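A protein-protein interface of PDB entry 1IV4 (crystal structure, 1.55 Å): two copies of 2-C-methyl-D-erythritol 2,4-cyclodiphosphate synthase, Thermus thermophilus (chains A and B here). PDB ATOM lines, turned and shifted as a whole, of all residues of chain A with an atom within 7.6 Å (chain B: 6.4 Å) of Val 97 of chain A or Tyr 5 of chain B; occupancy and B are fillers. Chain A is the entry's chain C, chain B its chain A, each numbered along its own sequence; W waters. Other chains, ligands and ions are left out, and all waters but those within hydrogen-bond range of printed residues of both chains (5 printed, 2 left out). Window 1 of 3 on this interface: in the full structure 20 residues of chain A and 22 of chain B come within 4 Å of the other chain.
The backbone NH of Tyr 5 of chain B sits at hydrogen-bond distance from the side-chain hydroxyl of Ser 95 of chain A (2.8 Å). The side-chain hydroxyl (OG) of Ser 50 of chain B sits at hydrogen-bond distance from the backbone carbonyl oxygen (O) of Gly 128 of chain A (3.0 Å). The side-chain carboxylate of Glu 7 of chain B lies within salt-bridge range of the guanidinium group of Arg 145 of chain A. The side-chain hydroxyl (OG) of Ser 50 of chain B is in hydrogen-bond range of the side-chain hydroxyl (OG) of Ser 95 of chain A (2.7 Å). The side-chain hydroxyl of Tyr 5 of chain A lies within hydrogen-bond range of the side-chain hydroxyl of Tyr 5 of chain B, 3.3 Å away.
The backbone NH (N) of Ala 146 of chain B lies within hydrogen-bond range of the backbone carbonyl oxygen (O) of Gly 6 of chain B, at 2.8 Å. NE of Arg 145 of chain A is in salt-bridge range of OE1 of Glu 7 of chain A, 3.0 Å away. O of Ser 95 of chain A sits at hydrogen-bond distance from N of Val 147 of chain A, 2.9 Å away. N of Val 148 of chain B is in hydrogen-bond range of O of Gly 4 of chain B. OE1 of Glu 7 of chain B is in salt-bridge range of NE of Arg 145 of chain B (3.0 Å).
Among the printed residues, merely in contact across the chains: Ser 95 of chain A with Gly 4 of chain B, Val 97 of chain A with Tyr 5 of chain B, Val 97 of chain A with Gly 6 of chain B, Val 97 of chain A with Glu 7 of chain B, Leu 129 of chain A with Ser 50 of chain B, Lys 132 of chain A with Glu 7 of chain B, Lys 132 of chain A with Asp 46 of chain B, Arg 145 of chain A with Tyr 5 of chain B, Arg 145 of chain A with Arg 145 of chain B and Val 147 of chain A with Ile 3 of chain B.
Ala 94 of chain A touches none of the printed residues of chain B. Of chain B, only Tyr 5, Gly 6 and Glu 7 come within 4 Å of Val 97 of chain A. Of the printed residues of chain B, Leu 129 of chain A touches Ser 50 (3.9 Å). Gln 143 of chain A touches none of the printed residues of chain B. Of chain A, only Tyr 5, Ser 95, Val 97 and Arg 145 come within 4 Å of Tyr 5 of chain B. Of the printed residues of chain A, Gly 6 of chain B touches Val 97 (3.9 Å). Of the printed residues of chain A, Glu 7 of chain B touches Val 97 (3.8 Å), Lys 132 (3.0 Å) and Arg 145 (3.0 Å). The nearest printed residue of chain B that does not touch Val 97 of chain A is Asp 46 of chain B (6.2 Å). The nearest residue of chain A that does not touch Tyr 5 of chain B is Val 147 of chain A (4.1 Å). The nearest printed residue of chain B that does not touch Leu 129 of chain A is Asp 46 of chain B (6.9 Å).
Of the 27 printed residues of chain A, 8 touch a printed residue of chain B. Among the printed residues, 15 pairs touch across the chains.
Arg 145 of chain A touches Tyr 5 of chain B, but with the chains exchanged Tyr 5 of chain A does not touch Arg 145 of chain B (5.2 Å). Arg 145 of chain B touches its own counterpart, Arg 145 of chain A. Positions printed for both chains: 5, 6, 7, 43, 145, 146, 147 and 148. Of the 15 pairs that touch across the chains among the printed residues, 2 have their exchanged pair printed and touching as well.
Water W3 bridges O of Ser 50 of chain B (2.7 Å) and N of Gly 128 of chain A (3.3 Å). Water W2 lies within hydrogen-bond range of the side-chain carboxylate (OD2) of Asp 46 of chain B (2.8 Å), the side-chain hydroxyl (OG1) of Thr 130 of chain A (2.8 Å) and the backbone NH (N) of Glu 7 of chain B (3.0 Å).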
ATOM      1  N   TYR A   5       7.595 -30.574  18.065  1.00  0.00           N
ATOM      2  CA  TYR A   5       6.813 -29.579  17.358  1.00  0.00           C
ATOM      3  C   TYR A   5       7.377 -29.425  15.948  1.00  0.00           C
ATOM      4  O   TYR A   5       8.602 -29.309  15.792  1.00  0.00           O
ATOM      5  CB  TYR A   5       6.813 -28.244  18.104  1.00  0.00           C
ATOM      6  CG  TYR A   5       5.927 -27.221  17.424  1.00  0.00           C
ATOM      7  CD1 TYR A   5       4.546 -27.326  17.386  1.00  0.00           C
ATOM      8  CD2 TYR A   5       6.512 -26.119  16.817  1.00  0.00           C
ATOM      9  CE1 TYR A   5       3.743 -26.379  16.768  1.00  0.00           C
ATOM     10  CE2 TYR A   5       5.721 -25.180  16.193  1.00  0.00           C
ATOM     11  CZ  TYR A   5       4.356 -25.305  16.160  1.00  0.00           C
ATOM     12  OH  TYR A   5       3.614 -24.330  15.520  1.00  0.00           O
ATOM     13  N   GLY A   6       6.549 -29.436  14.915  1.00  0.00           N
ATOM     14  CA  GLY A   6       7.067 -29.299  13.549  1.00  0.00           C
ATOM     15  C   GLY A   6       6.102 -28.490  12.700  1.00  0.00           C
ATOM     16  O   GLY A   6       4.899 -28.423  12.993  1.00  0.00           O
ATOM     17  N   GLU A   7       6.619 -27.902  11.636  1.00  0.00           N
ATOM     18  CA  GLU A   7       5.819 -27.087  10.724  1.00  0.00           C
ATOM     19  C   GLU A   7       6.230 -27.375   9.283  1.00  0.00           C
ATOM     20  O   GLU A   7       7.394 -27.741   9.021  1.00  0.00           O
ATOM     21  CB  GLU A   7       6.011 -25.584  10.959  1.00  0.00           C
ATOM     22  CG  GLU A   7       5.585 -25.092  12.330  1.00  0.00           C
ATOM     23  CD  GLU A   7       5.628 -23.567  12.366  1.00  0.00           C
ATOM     24  OE1 GLU A   7       5.198 -22.953  11.358  1.00  0.00           O
ATOM     25  OE2 GLU A   7       6.075 -23.037  13.385  1.00  0.00           O
ATOM     26  N   ASP A   8       5.301 -27.175   8.362  1.00  0.00           N
ATOM     27  CA  ASP A   8       5.662 -27.177   6.947  1.00  0.00           C
ATOM     28  C   ASP A   8       4.730 -26.267   6.165  1.00  0.00           C
ATOM     29  O   ASP A   8       3.618 -25.976   6.607  1.00  0.00           O
ATOM     30  CB  ASP A   8       5.629 -28.567   6.316  1.00  0.00           C
ATOM     31  CG  ASP A   8       6.401 -28.611   4.983  1.00  0.00           C
ATOM     32  OD1 ASP A   8       7.283 -27.761   4.759  1.00  0.00           O
ATOM     33  OD2 ASP A   8       6.019 -29.460   4.160  1.00  0.00           O
ATOM     34  N   ALA A  39       2.424 -31.214   3.191  1.00  0.00           N
ATOM     35  CA  ALA A  39       2.785 -30.417   4.360  1.00  0.00           C
ATOM     36  C   ALA A  39       2.457 -31.141   5.661  1.00  0.00           C
ATOM     37  O   ALA A  39       3.134 -30.970   6.677  1.00  0.00           O
ATOM     38  CB  ALA A  39       2.049 -29.089   4.338  1.00  0.00           C
ATOM     39  N   ALA A  40       1.364 -31.919   5.641  1.00  0.00           N
ATOM     40  CA  ALA A  40       0.989 -32.620   6.870  1.00  0.00           C
ATOM     41  C   ALA A  40       2.041 -33.655   7.232  1.00  0.00           C
ATOM     42  O   ALA A  40       2.539 -33.697   8.352  1.00  0.00           O
ATOM     43  CB  ALA A  40      -0.372 -33.283   6.733  1.00  0.00           C
ATOM     44  N   ALA A  43       5.358 -31.893   8.386  1.00  0.00           N
ATOM     45  CA  ALA A  43       5.298 -31.334   9.741  1.00  0.00           C
ATOM     46  C   ALA A  43       5.401 -32.418  10.800  1.00  0.00           C
ATOM     47  O   ALA A  43       6.118 -32.257  11.806  1.00  0.00           O
ATOM     48  CB  ALA A  43       3.986 -30.565   9.917  1.00  0.00           C
ATOM     49  N   ALA A  94      -0.660 -37.585  17.997  1.00  0.00           N
ATOM     50  CA  ALA A  94      -0.258 -36.538  17.044  1.00  0.00           C
ATOM     51  C   ALA A  94      -1.438 -35.581  16.867  1.00  0.00           C
ATOM     52  O   ALA A  94      -2.577 -36.032  16.640  1.00  0.00           O
ATOM     53  CB  ALA A  94       0.189 -37.086  15.707  1.00  0.00           C
ATOM     54  N   SER A  95      -1.167 -34.293  17.013  1.00  0.00           N
ATOM     55  CA  SER A  95      -2.262 -33.312  16.915  1.00  0.00           C
ATOM     56  C   SER A  95      -1.771 -32.256  15.950  1.00  0.00           C
ATOM     57  O   SER A  95      -0.701 -31.685  16.178  1.00  0.00           O
ATOM     58  CB  SER A  95      -2.606 -32.728  18.283  1.00  0.00           C
ATOM     59  OG  SER A  95      -3.620 -31.737  18.248  1.00  0.00           O
ATOM     60  N   LEU A  96      -2.527 -32.018  14.870  1.00  0.00           N
ATOM     61  CA  LEU A  96      -1.986 -31.082  13.883  1.00  0.00           C
ATOM     62  C   LEU A  96      -3.116 -30.283  13.226  1.00  0.00           C
ATOM     63  O   LEU A  96      -4.262 -30.721  13.275  1.00  0.00           O
ATOM     64  CB  LEU A  96      -1.166 -31.804  12.812  1.00  0.00           C
ATOM     65  CG  LEU A  96      -1.917 -32.662  11.807  1.00  0.00           C
ATOM     66  CD1 LEU A  96      -1.071 -32.987  10.581  1.00  0.00           C
ATOM     67  CD2 LEU A  96      -2.412 -33.977  12.402  1.00  0.00           C
ATOM     68  N   VAL A  97      -2.742 -29.132  12.690  1.00  0.00           N
ATOM     69  CA  VAL A  97      -3.701 -28.203  12.091  1.00  0.00           C
ATOM     70  C   VAL A  97      -3.277 -27.955  10.640  1.00  0.00           C
ATOM     71  O   VAL A  97      -2.122 -27.595  10.436  1.00  0.00           O
ATOM     72  CB  VAL A  97      -3.731 -26.861  12.824  1.00  0.00           C
ATOM     73  CG1 VAL A  97      -4.683 -25.889  12.107  1.00  0.00           C
ATOM     74  CG2 VAL A  97      -4.142 -27.027  14.277  1.00  0.00           C
ATOM     75  N   LEU A  98      -4.177 -28.165   9.687  1.00  0.00           N
ATOM     76  CA  LEU A  98      -3.887 -27.840   8.297  1.00  0.00           C
ATOM     77  C   LEU A  98      -4.571 -26.521   7.944  1.00  0.00           C
ATOM     78  O   LEU A  98      -5.763 -26.448   8.219  1.00  0.00           O
ATOM     79  CB  LEU A  98      -4.384 -28.951   7.371  1.00  0.00           C
ATOM     80  CG  LEU A  98      -3.871 -30.353   7.711  1.00  0.00           C
ATOM     81  CD1 LEU A  98      -4.389 -31.344   6.670  1.00  0.00           C
ATOM     82  CD2 LEU A  98      -2.355 -30.359   7.809  1.00  0.00           C
ATOM     83  N   THR A  99      -3.822 -25.583   7.406  1.00  0.00           N
ATOM     84  CA  THR A  99      -4.359 -24.302   6.973  1.00  0.00           C
ATOM     85  C   THR A  99      -4.342 -24.243   5.445  1.00  0.00           C
ATOM     86  O   THR A  99      -3.307 -24.373   4.821  1.00  0.00           O
ATOM     87  CB  THR A  99      -3.584 -23.120   7.575  1.00  0.00           C
ATOM     88  OG1 THR A  99      -3.571 -23.252   8.999  1.00  0.00           O
ATOM     89  CG2 THR A  99      -4.318 -21.832   7.257  1.00  0.00           C
ATOM     90  N   LEU A 100      -5.554 -24.103   4.898  1.00  0.00           N
ATOM     91  CA  LEU A 100      -5.626 -23.875   3.457  1.00  0.00           C
ATOM     92  C   LEU A 100      -7.054 -23.473   3.087  1.00  0.00           C
ATOM     93  O   LEU A 100      -8.017 -23.931   3.710  1.00  0.00           O
ATOM     94  CB  LEU A 100      -5.173 -25.075   2.653  1.00  0.00           C
ATOM     95  CG  LEU A 100      -6.089 -26.285   2.731  1.00  0.00           C
ATOM     96  CD1 LEU A 100      -5.786 -27.250   1.593  1.00  0.00           C
ATOM     97  CD2 LEU A 100      -5.942 -26.961   4.084  1.00  0.00           C
ATOM     98  N   GLY A 128      -5.281 -36.166  16.134  1.00  0.00           N
ATOM     99  CA  GLY A 128      -6.053 -34.931  16.295  1.00  0.00           C
ATOM    100  C   GLY A 128      -5.875 -34.039  15.102  1.00  0.00           C
ATOM    101  O   GLY A 128      -4.894 -33.307  15.059  1.00  0.00           O
ATOM    102  N   LEU A 129      -6.783 -34.101  14.137  1.00  0.00           N
ATOM    103  CA  LEU A 129      -6.618 -33.366  12.893  1.00  0.00           C
ATOM    104  C   LEU A 129      -7.721 -32.309  12.833  1.00  0.00           C
ATOM    105  O   LEU A 129      -8.881 -32.648  13.052  1.00  0.00           O
ATOM    106  CB  LEU A 129      -6.694 -34.332  11.716  1.00  0.00           C
ATOM    107  CG  LEU A 129      -6.594 -33.743  10.307  1.00  0.00           C
ATOM    108  CD1 LEU A 129      -5.267 -33.065  10.007  1.00  0.00           C
ATOM    109  CD2 LEU A 129      -6.817 -34.864   9.277  1.00  0.00           C
ATOM    110  N   THR A 130      -7.341 -31.064  12.598  1.00  0.00           N
ATOM    111  CA  THR A 130      -8.280 -29.963  12.456  1.00  0.00           C
ATOM    112  C   THR A 130      -7.907 -29.169  11.202  1.00  0.00           C
ATOM    113  O   THR A 130      -6.735 -29.095  10.810  1.00  0.00           O
ATOM    114  CB  THR A 130      -8.361 -29.017  13.674  1.00  0.00           C
ATOM    115  OG1 THR A 130      -7.091 -28.408  13.902  1.00  0.00           O
ATOM    116  CG2 THR A 130      -8.739 -29.793  14.934  1.00  0.00           C
ATOM    117  N   PHE A 131      -8.923 -28.563  10.589  1.00  0.00           N
ATOM    118  CA  PHE A 131      -8.712 -27.778   9.384  1.00  0.00           C
ATOM    119  C   PHE A 131      -9.109 -26.310   9.545  1.00  0.00           C
ATOM    120  O   PHE A 131     -10.111 -26.095  10.223  1.00  0.00           O
ATOM    121  CB  PHE A 131      -9.573 -28.283   8.214  1.00  0.00           C
ATOM    122  CG  PHE A 131      -9.523 -29.783   8.051  1.00  0.00           C
ATOM    123  CD1 PHE A 131      -8.308 -30.432   7.966  1.00  0.00           C
ATOM    124  CD2 PHE A 131     -10.692 -30.516   7.991  1.00  0.00           C
ATOM    125  CE1 PHE A 131      -8.258 -31.807   7.849  1.00  0.00           C
ATOM    126  CE2 PHE A 131     -10.649 -31.890   7.892  1.00  0.00           C
ATOM    127  CZ  PHE A 131      -9.434 -32.543   7.819  1.00  0.00           C
ATOM    128  N   LYS A 132      -8.354 -25.414   8.898  1.00  0.00           N
ATOM    129  CA  LYS A 132      -8.819 -24.029   8.858  1.00  0.00           C
ATOM    130  C   LYS A 132      -8.473 -23.386   7.522  1.00  0.00           C
ATOM    131  O   LYS A 132      -7.568 -23.862   6.825  1.00  0.00           O
ATOM    132  CB  LYS A 132      -8.243 -23.159   9.980  1.00  0.00           C
ATOM    133  CG  LYS A 132      -7.983 -23.735  11.332  1.00  0.00           C
ATOM    134  CD  LYS A 132      -9.012 -23.456  12.399  1.00  0.00           C
ATOM    135  CE  LYS A 132      -9.665 -22.106  12.346  1.00  0.00           C
ATOM    136  NZ  LYS A 132     -11.125 -22.091  12.702  1.00  0.00           N
ATOM    137  N   THR A 133      -9.223 -22.319   7.203  1.00  0.00           N
ATOM    138  CA  THR A 133      -8.801 -21.478   6.078  1.00  0.00           C
ATOM    139  C   THR A 133      -7.803 -20.452   6.598  1.00  0.00           C
ATOM    140  O   THR A 133      -7.532 -20.412   7.793  1.00  0.00           O
ATOM    141  CB  THR A 133      -9.929 -20.699   5.381  1.00  0.00           C
ATOM    142  OG1 THR A 133     -10.469 -19.735   6.297  1.00  0.00           O
ATOM    143  CG2 THR A 133     -11.071 -21.638   5.040  1.00  0.00           C
ATOM    144  N   VAL A 142      -0.436 -24.032   1.328  1.00  0.00           N
ATOM    145  CA  VAL A 142      -0.930 -24.931   2.374  1.00  0.00           C
ATOM    146  C   VAL A 142       0.098 -24.916   3.507  1.00  0.00           C
ATOM    147  O   VAL A 142       1.296 -24.920   3.251  1.00  0.00           O
ATOM    148  CB  VAL A 142      -1.169 -26.340   1.849  1.00  0.00           C
ATOM    149  CG1 VAL A 142       0.103 -26.868   1.201  1.00  0.00           C
ATOM    150  CG2 VAL A 142      -1.662 -27.234   2.980  1.00  0.00           C
ATOM    151  N   GLN A 143      -0.391 -24.883   4.728  1.00  0.00           N
ATOM    152  CA  GLN A 143       0.433 -24.808   5.926  1.00  0.00           C
ATOM    153  C   GLN A 143      -0.010 -25.896   6.898  1.00  0.00           C
ATOM    154  O   GLN A 143      -1.189 -26.229   7.005  1.00  0.00           O
ATOM    155  CB  GLN A 143       0.285 -23.468   6.624  1.00  0.00           C
ATOM    156  CG  GLN A 143       0.655 -22.273   5.754  1.00  0.00           C
ATOM    157  CD  GLN A 143       0.250 -20.981   6.436  1.00  0.00           C
ATOM    158  OE1 GLN A 143      -0.799 -20.405   6.151  1.00  0.00           O
ATOM    159  NE2 GLN A 143       1.111 -20.540   7.357  1.00  0.00           N
ATOM    160  N   ALA A 144       0.980 -26.452   7.616  1.00  0.00           N
ATOM    161  CA  ALA A 144       0.689 -27.462   8.614  1.00  0.00           C
ATOM    162  C   ALA A 144       1.570 -27.274   9.858  1.00  0.00           C
ATOM    163  O   ALA A 144       2.752 -26.958   9.682  1.00  0.00           O
ATOM    164  CB  ALA A 144       0.948 -28.886   8.102  1.00  0.00           C
ATOM    165  N   ARG A 145       0.971 -27.448  11.023  1.00  0.00           N
ATOM    166  CA  ARG A 145       1.753 -27.303  12.274  1.00  0.00           C
ATOM    167  C   ARG A 145       1.343 -28.475  13.145  1.00  0.00           C
ATOM    168  O   ARG A 145       0.147 -28.723  13.283  1.00  0.00           O
ATOM    169  CB  ARG A 145       1.512 -25.962  12.979  1.00  0.00           C
ATOM    170  CG  ARG A 145       1.842 -24.775  12.090  1.00  0.00           C
ATOM    171  CD  ARG A 145       1.949 -23.411  12.756  1.00  0.00           C
ATOM    172  NE  ARG A 145       2.322 -22.382  11.776  1.00  0.00           N
ATOM    173  CZ  ARG A 145       1.447 -21.715  11.031  1.00  0.00           C
ATOM    174  NH1 ARG A 145       0.140 -21.936  11.129  1.00  0.00           N
ATOM    175  NH2 ARG A 145       1.895 -20.806  10.172  1.00  0.00           N
ATOM    176  N   ALA A 146       2.332 -29.185  13.702  1.00  0.00           N
ATOM    177  CA  ALA A 146       2.007 -30.409  14.402  1.00  0.00           C
ATOM    178  C   ALA A 146       2.726 -30.556  15.736  1.00  0.00           C
ATOM    179  O   ALA A 146       3.884 -30.156  15.796  1.00  0.00           O
ATOM    180  CB  ALA A 146       2.421 -31.605  13.543  1.00  0.00           C
ATOM    181  N   VAL A 147       2.050 -31.120  16.722  1.00  0.00           N
ATOM    182  CA  VAL A 147       2.707 -31.559  17.945  1.00  0.00           C
ATOM    183  C   VAL A 147       2.599 -33.069  18.076  1.00  0.00           C
ATOM    184  O   VAL A 147       1.514 -33.615  17.842  1.00  0.00           O
ATOM    185  CB  VAL A 147       2.031 -30.970  19.191  1.00  0.00           C
ATOM    186  CG1 VAL A 147       2.648 -31.519  20.464  1.00  0.00           C
ATOM    187  CG2 VAL A 147       2.093 -29.450  19.134  1.00  0.00           C
ATOM    188  N   VAL A 148       3.678 -33.720  18.478  1.00  0.00           N
ATOM    189  CA  VAL A 148       3.594 -35.134  18.822  1.00  0.00           C
ATOM    190  C   VAL A 148       3.935 -35.373  20.293  1.00  0.00           C
ATOM    191  O   VAL A 148       4.724 -34.608  20.868  1.00  0.00           O
ATOM    192  CB  VAL A 148       4.528 -35.988  17.958  1.00  0.00           C
ATOM    193  CG1 VAL A 148       4.051 -35.893  16.519  1.00  0.00           C
ATOM    194  CG2 VAL A 148       5.986 -35.561  18.057  1.00  0.00           C
ATOM    195  N   ILE B   3      -2.524 -34.474  24.635  1.00  0.00           N
ATOM    196  CA  ILE B   3      -2.232 -33.129  24.165  1.00  0.00           C
ATOM    197  C   ILE B   3      -3.121 -32.833  22.960  1.00  0.00           C
ATOM    198  O   ILE B   3      -3.543 -33.693  22.206  1.00  0.00           O
ATOM    199  CB  ILE B   3      -0.763 -32.933  23.756  1.00  0.00           C
ATOM    200  CG1 ILE B   3      -0.301 -31.493  23.504  1.00  0.00           C
ATOM    201  CG2 ILE B   3      -0.404 -33.748  22.517  1.00  0.00           C
ATOM    202  CD1 ILE B   3       1.218 -31.370  23.545  1.00  0.00           C
ATOM    203  N   GLY B   4      -3.384 -31.528  22.805  1.00  0.00           N
ATOM    204  CA  GLY B   4      -4.091 -31.100  21.602  1.00  0.00           C
ATOM    205  C   GLY B   4      -3.567 -29.732  21.167  1.00  0.00           C
ATOM    206  O   GLY B   4      -3.137 -28.950  21.999  1.00  0.00           O
ATOM    207  N   TYR B   5      -3.593 -29.488  19.872  1.00  0.00           N
ATOM    208  CA  TYR B   5      -3.090 -28.240  19.308  1.00  0.00           C
ATOM    209  C   TYR B   5      -4.148 -27.629  18.402  1.00  0.00           C
ATOM    210  O   TYR B   5      -4.730 -28.340  17.583  1.00  0.00           O
ATOM    211  CB  TYR B   5      -1.808 -28.519  18.531  1.00  0.00           C
ATOM    212  CG  TYR B   5      -1.215 -27.299  17.866  1.00  0.00           C
ATOM    213  CD1 TYR B   5      -0.678 -26.295  18.669  1.00  0.00           C
ATOM    214  CD2 TYR B   5      -1.173 -27.166  16.485  1.00  0.00           C
ATOM    215  CE1 TYR B   5      -0.117 -25.171  18.101  1.00  0.00           C
ATOM    216  CE2 TYR B   5      -0.617 -26.030  15.902  1.00  0.00           C
ATOM    217  CZ  TYR B   5      -0.104 -25.054  16.725  1.00  0.00           C
ATOM    218  OH  TYR B   5       0.463 -23.904  16.203  1.00  0.00           O
ATOM    219  N   GLY B   6      -4.416 -26.336  18.522  1.00  0.00           N
ATOM    220  CA  GLY B   6      -5.457 -25.741  17.689  1.00  0.00           C
ATOM    221  C   GLY B   6      -5.075 -24.325  17.309  1.00  0.00           C
ATOM    222  O   GLY B   6      -4.269 -23.665  17.978  1.00  0.00           O
ATOM    223  N   GLU B   7      -5.654 -23.868  16.199  1.00  0.00           N
ATOM    224  CA  GLU B   7      -5.377 -22.527  15.683  1.00  0.00           C
ATOM    225  C   GLU B   7      -6.678 -21.856  15.237  1.00  0.00           C
ATOM    226  O   GLU B   7      -7.630 -22.555  14.894  1.00  0.00           O
ATOM    227  CB  GLU B   7      -4.458 -22.592  14.467  1.00  0.00           C
ATOM    228  CG  GLU B   7      -3.046 -23.134  14.683  1.00  0.00           C
ATOM    229  CD  GLU B   7      -2.215 -22.901  13.426  1.00  0.00           C
ATOM    230  OE1 GLU B   7      -2.313 -21.781  12.843  1.00  0.00           O
ATOM    231  OE2 GLU B   7      -1.441 -23.779  13.019  1.00  0.00           O
ATOM    232  N   ALA B  43      -9.500 -21.358  18.945  1.00  0.00           N
ATOM    233  CA  ALA B  43      -8.275 -22.172  18.976  1.00  0.00           C
ATOM    234  C   ALA B  43      -8.283 -23.153  20.145  1.00  0.00           C
ATOM    235  O   ALA B  43      -7.909 -24.323  20.011  1.00  0.00           O
ATOM    236  CB  ALA B  43      -7.021 -21.298  19.027  1.00  0.00           C
ATOM    237  N   ASP B  46     -10.810 -26.014  19.335  1.00  0.00           N
ATOM    238  CA  ASP B  46     -10.228 -26.983  18.422  1.00  0.00           C
ATOM    239  C   ASP B  46      -9.139 -27.796  19.124  1.00  0.00           C
ATOM    240  O   ASP B  46      -9.051 -28.997  18.862  1.00  0.00           O
ATOM    241  CB  ASP B  46      -9.619 -26.325  17.172  1.00  0.00           C
ATOM    242  CG  ASP B  46     -10.622 -26.162  16.040  1.00  0.00           C
ATOM    243  OD1 ASP B  46     -11.756 -26.685  16.186  1.00  0.00           O
ATOM    244  OD2 ASP B  46     -10.217 -25.520  15.054  1.00  0.00           O
ATOM    245  N   ALA B  47      -8.326 -27.157  19.971  1.00  0.00           N
ATOM    246  CA  ALA B  47      -7.309 -27.930  20.698  1.00  0.00           C
ATOM    247  C   ALA B  47      -7.926 -29.003  21.590  1.00  0.00           C
ATOM    248  O   ALA B  47      -7.441 -30.148  21.602  1.00  0.00           O
ATOM    249  CB  ALA B  47      -6.409 -27.009  21.505  1.00  0.00           C
ATOM    250  N   LEU B  48      -9.000 -28.688  22.324  1.00  0.00           N
ATOM    251  CA  LEU B  48      -9.658 -29.698  23.155  1.00  0.00           C
ATOM    252  C   LEU B  48     -10.220 -30.840  22.316  1.00  0.00           C
ATOM    253  O   LEU B  48     -10.023 -32.010  22.646  1.00  0.00           O
ATOM    254  CB  LEU B  48     -10.797 -29.098  23.981  1.00  0.00           C
ATOM    255  CG  LEU B  48     -10.343 -28.078  25.035  1.00  0.00           C
ATOM    256  CD1 LEU B  48     -11.532 -27.237  25.478  1.00  0.00           C
ATOM    257  CD2 LEU B  48      -9.668 -28.803  26.183  1.00  0.00           C
ATOM    258  N   SER B  50      -9.308 -31.732  19.347  1.00  0.00           N
ATOM    259  CA  SER B  50      -8.193 -32.437  18.730  1.00  0.00           C
ATOM    260  C   SER B  50      -7.597 -33.460  19.705  1.00  0.00           C
ATOM    261  O   SER B  50      -7.167 -34.514  19.249  1.00  0.00           O
ATOM    262  CB  SER B  50      -7.107 -31.447  18.303  1.00  0.00           C
ATOM    263  OG  SER B  50      -6.208 -32.047  17.394  1.00  0.00           O
ATOM    264  N   ALA B  51      -7.577 -33.150  20.995  1.00  0.00           N
ATOM    265  CA  ALA B  51      -6.958 -34.025  21.988  1.00  0.00           C
ATOM    266  C   ALA B  51      -7.692 -35.361  22.056  1.00  0.00           C
ATOM    267  O   ALA B  51      -7.116 -36.317  22.598  1.00  0.00           O
ATOM    268  CB  ALA B  51      -6.912 -33.354  23.354  1.00  0.00           C
ATOM    269  N   ARG B 145      -2.977 -19.403  18.569  1.00  0.00           N
ATOM    270  CA  ARG B 145      -2.490 -20.782  18.499  1.00  0.00           C
ATOM    271  C   ARG B 145      -2.448 -21.306  19.927  1.00  0.00           C
ATOM    272  O   ARG B 145      -1.997 -20.587  20.824  1.00  0.00           O
ATOM    273  CB  ARG B 145      -1.153 -20.803  17.753  1.00  0.00           C
ATOM    274  CG  ARG B 145      -1.295 -20.302  16.301  1.00  0.00           C
ATOM    275  CD  ARG B 145      -0.058 -20.600  15.469  1.00  0.00           C
ATOM    276  NE  ARG B 145      -0.172 -20.060  14.105  1.00  0.00           N
ATOM    277  CZ  ARG B 145       0.139 -18.808  13.787  1.00  0.00           C
ATOM    278  NH1 ARG B 145       0.585 -17.940  14.690  1.00  0.00           N
ATOM    279  NH2 ARG B 145       0.009 -18.391  12.527  1.00  0.00           N
ATOM    280  N   ALA B 146      -2.938 -22.500  20.178  1.00  0.00           N
ATOM    281  CA  ALA B 146      -3.161 -22.963  21.553  1.00  0.00           C
ATOM    282  C   ALA B 146      -2.745 -24.425  21.715  1.00  0.00           C
ATOM    283  O   ALA B 146      -2.993 -25.233  20.830  1.00  0.00           O
ATOM    284  CB  ALA B 146      -4.603 -22.818  22.008  1.00  0.00           C
ATOM    285  N   VAL B 147      -2.105 -24.741  22.832  1.00  0.00           N
ATOM    286  CA  VAL B 147      -1.879 -26.144  23.192  1.00  0.00           C
ATOM    287  C   VAL B 147      -2.605 -26.414  24.496  1.00  0.00           C
ATOM    288  O   VAL B 147      -2.570 -25.604  25.435  1.00  0.00           O
ATOM    289  CB  VAL B 147      -0.385 -26.450  23.387  1.00  0.00           C
ATOM    290  CG1 VAL B 147      -0.178 -27.903  23.778  1.00  0.00           C
ATOM    291  CG2 VAL B 147       0.405 -26.131  22.139  1.00  0.00           C
ATOM    292  N   VAL B 148      -3.265 -27.560  24.544  1.00  0.00           N
ATOM    293  CA  VAL B 148      -3.847 -27.999  25.818  1.00  0.00           C
ATOM    294  C   VAL B 148      -3.235 -29.323  26.278  1.00  0.00           C
ATOM    295  O   VAL B 148      -2.799 -30.119  25.449  1.00  0.00           O
ATOM    296  CB  VAL B 148      -5.380 -28.150  25.744  1.00  0.00           C
ATOM    297  CG1 VAL B 148      -5.985 -26.778  25.480  1.00  0.00           C
ATOM    298  CG2 VAL B 148      -5.753 -29.192  24.705  1.00  0.00           C
HETATM  299  O   HOH W   1     -11.183 -25.217  12.463  1.00  0.00           O
HETATM  300  O   HOH W   2      -7.473 -25.732  14.672  1.00  0.00           O
HETATM  301  O   HOH W   3      -6.026 -37.004  19.236  1.00  0.00           O
HETATM  302  O   HOH W   4      -1.739 -24.773  10.202  1.00  0.00           O
HETATM  303  O   HOH W   5      -3.685 -21.130  10.598  1.00  0.00           O
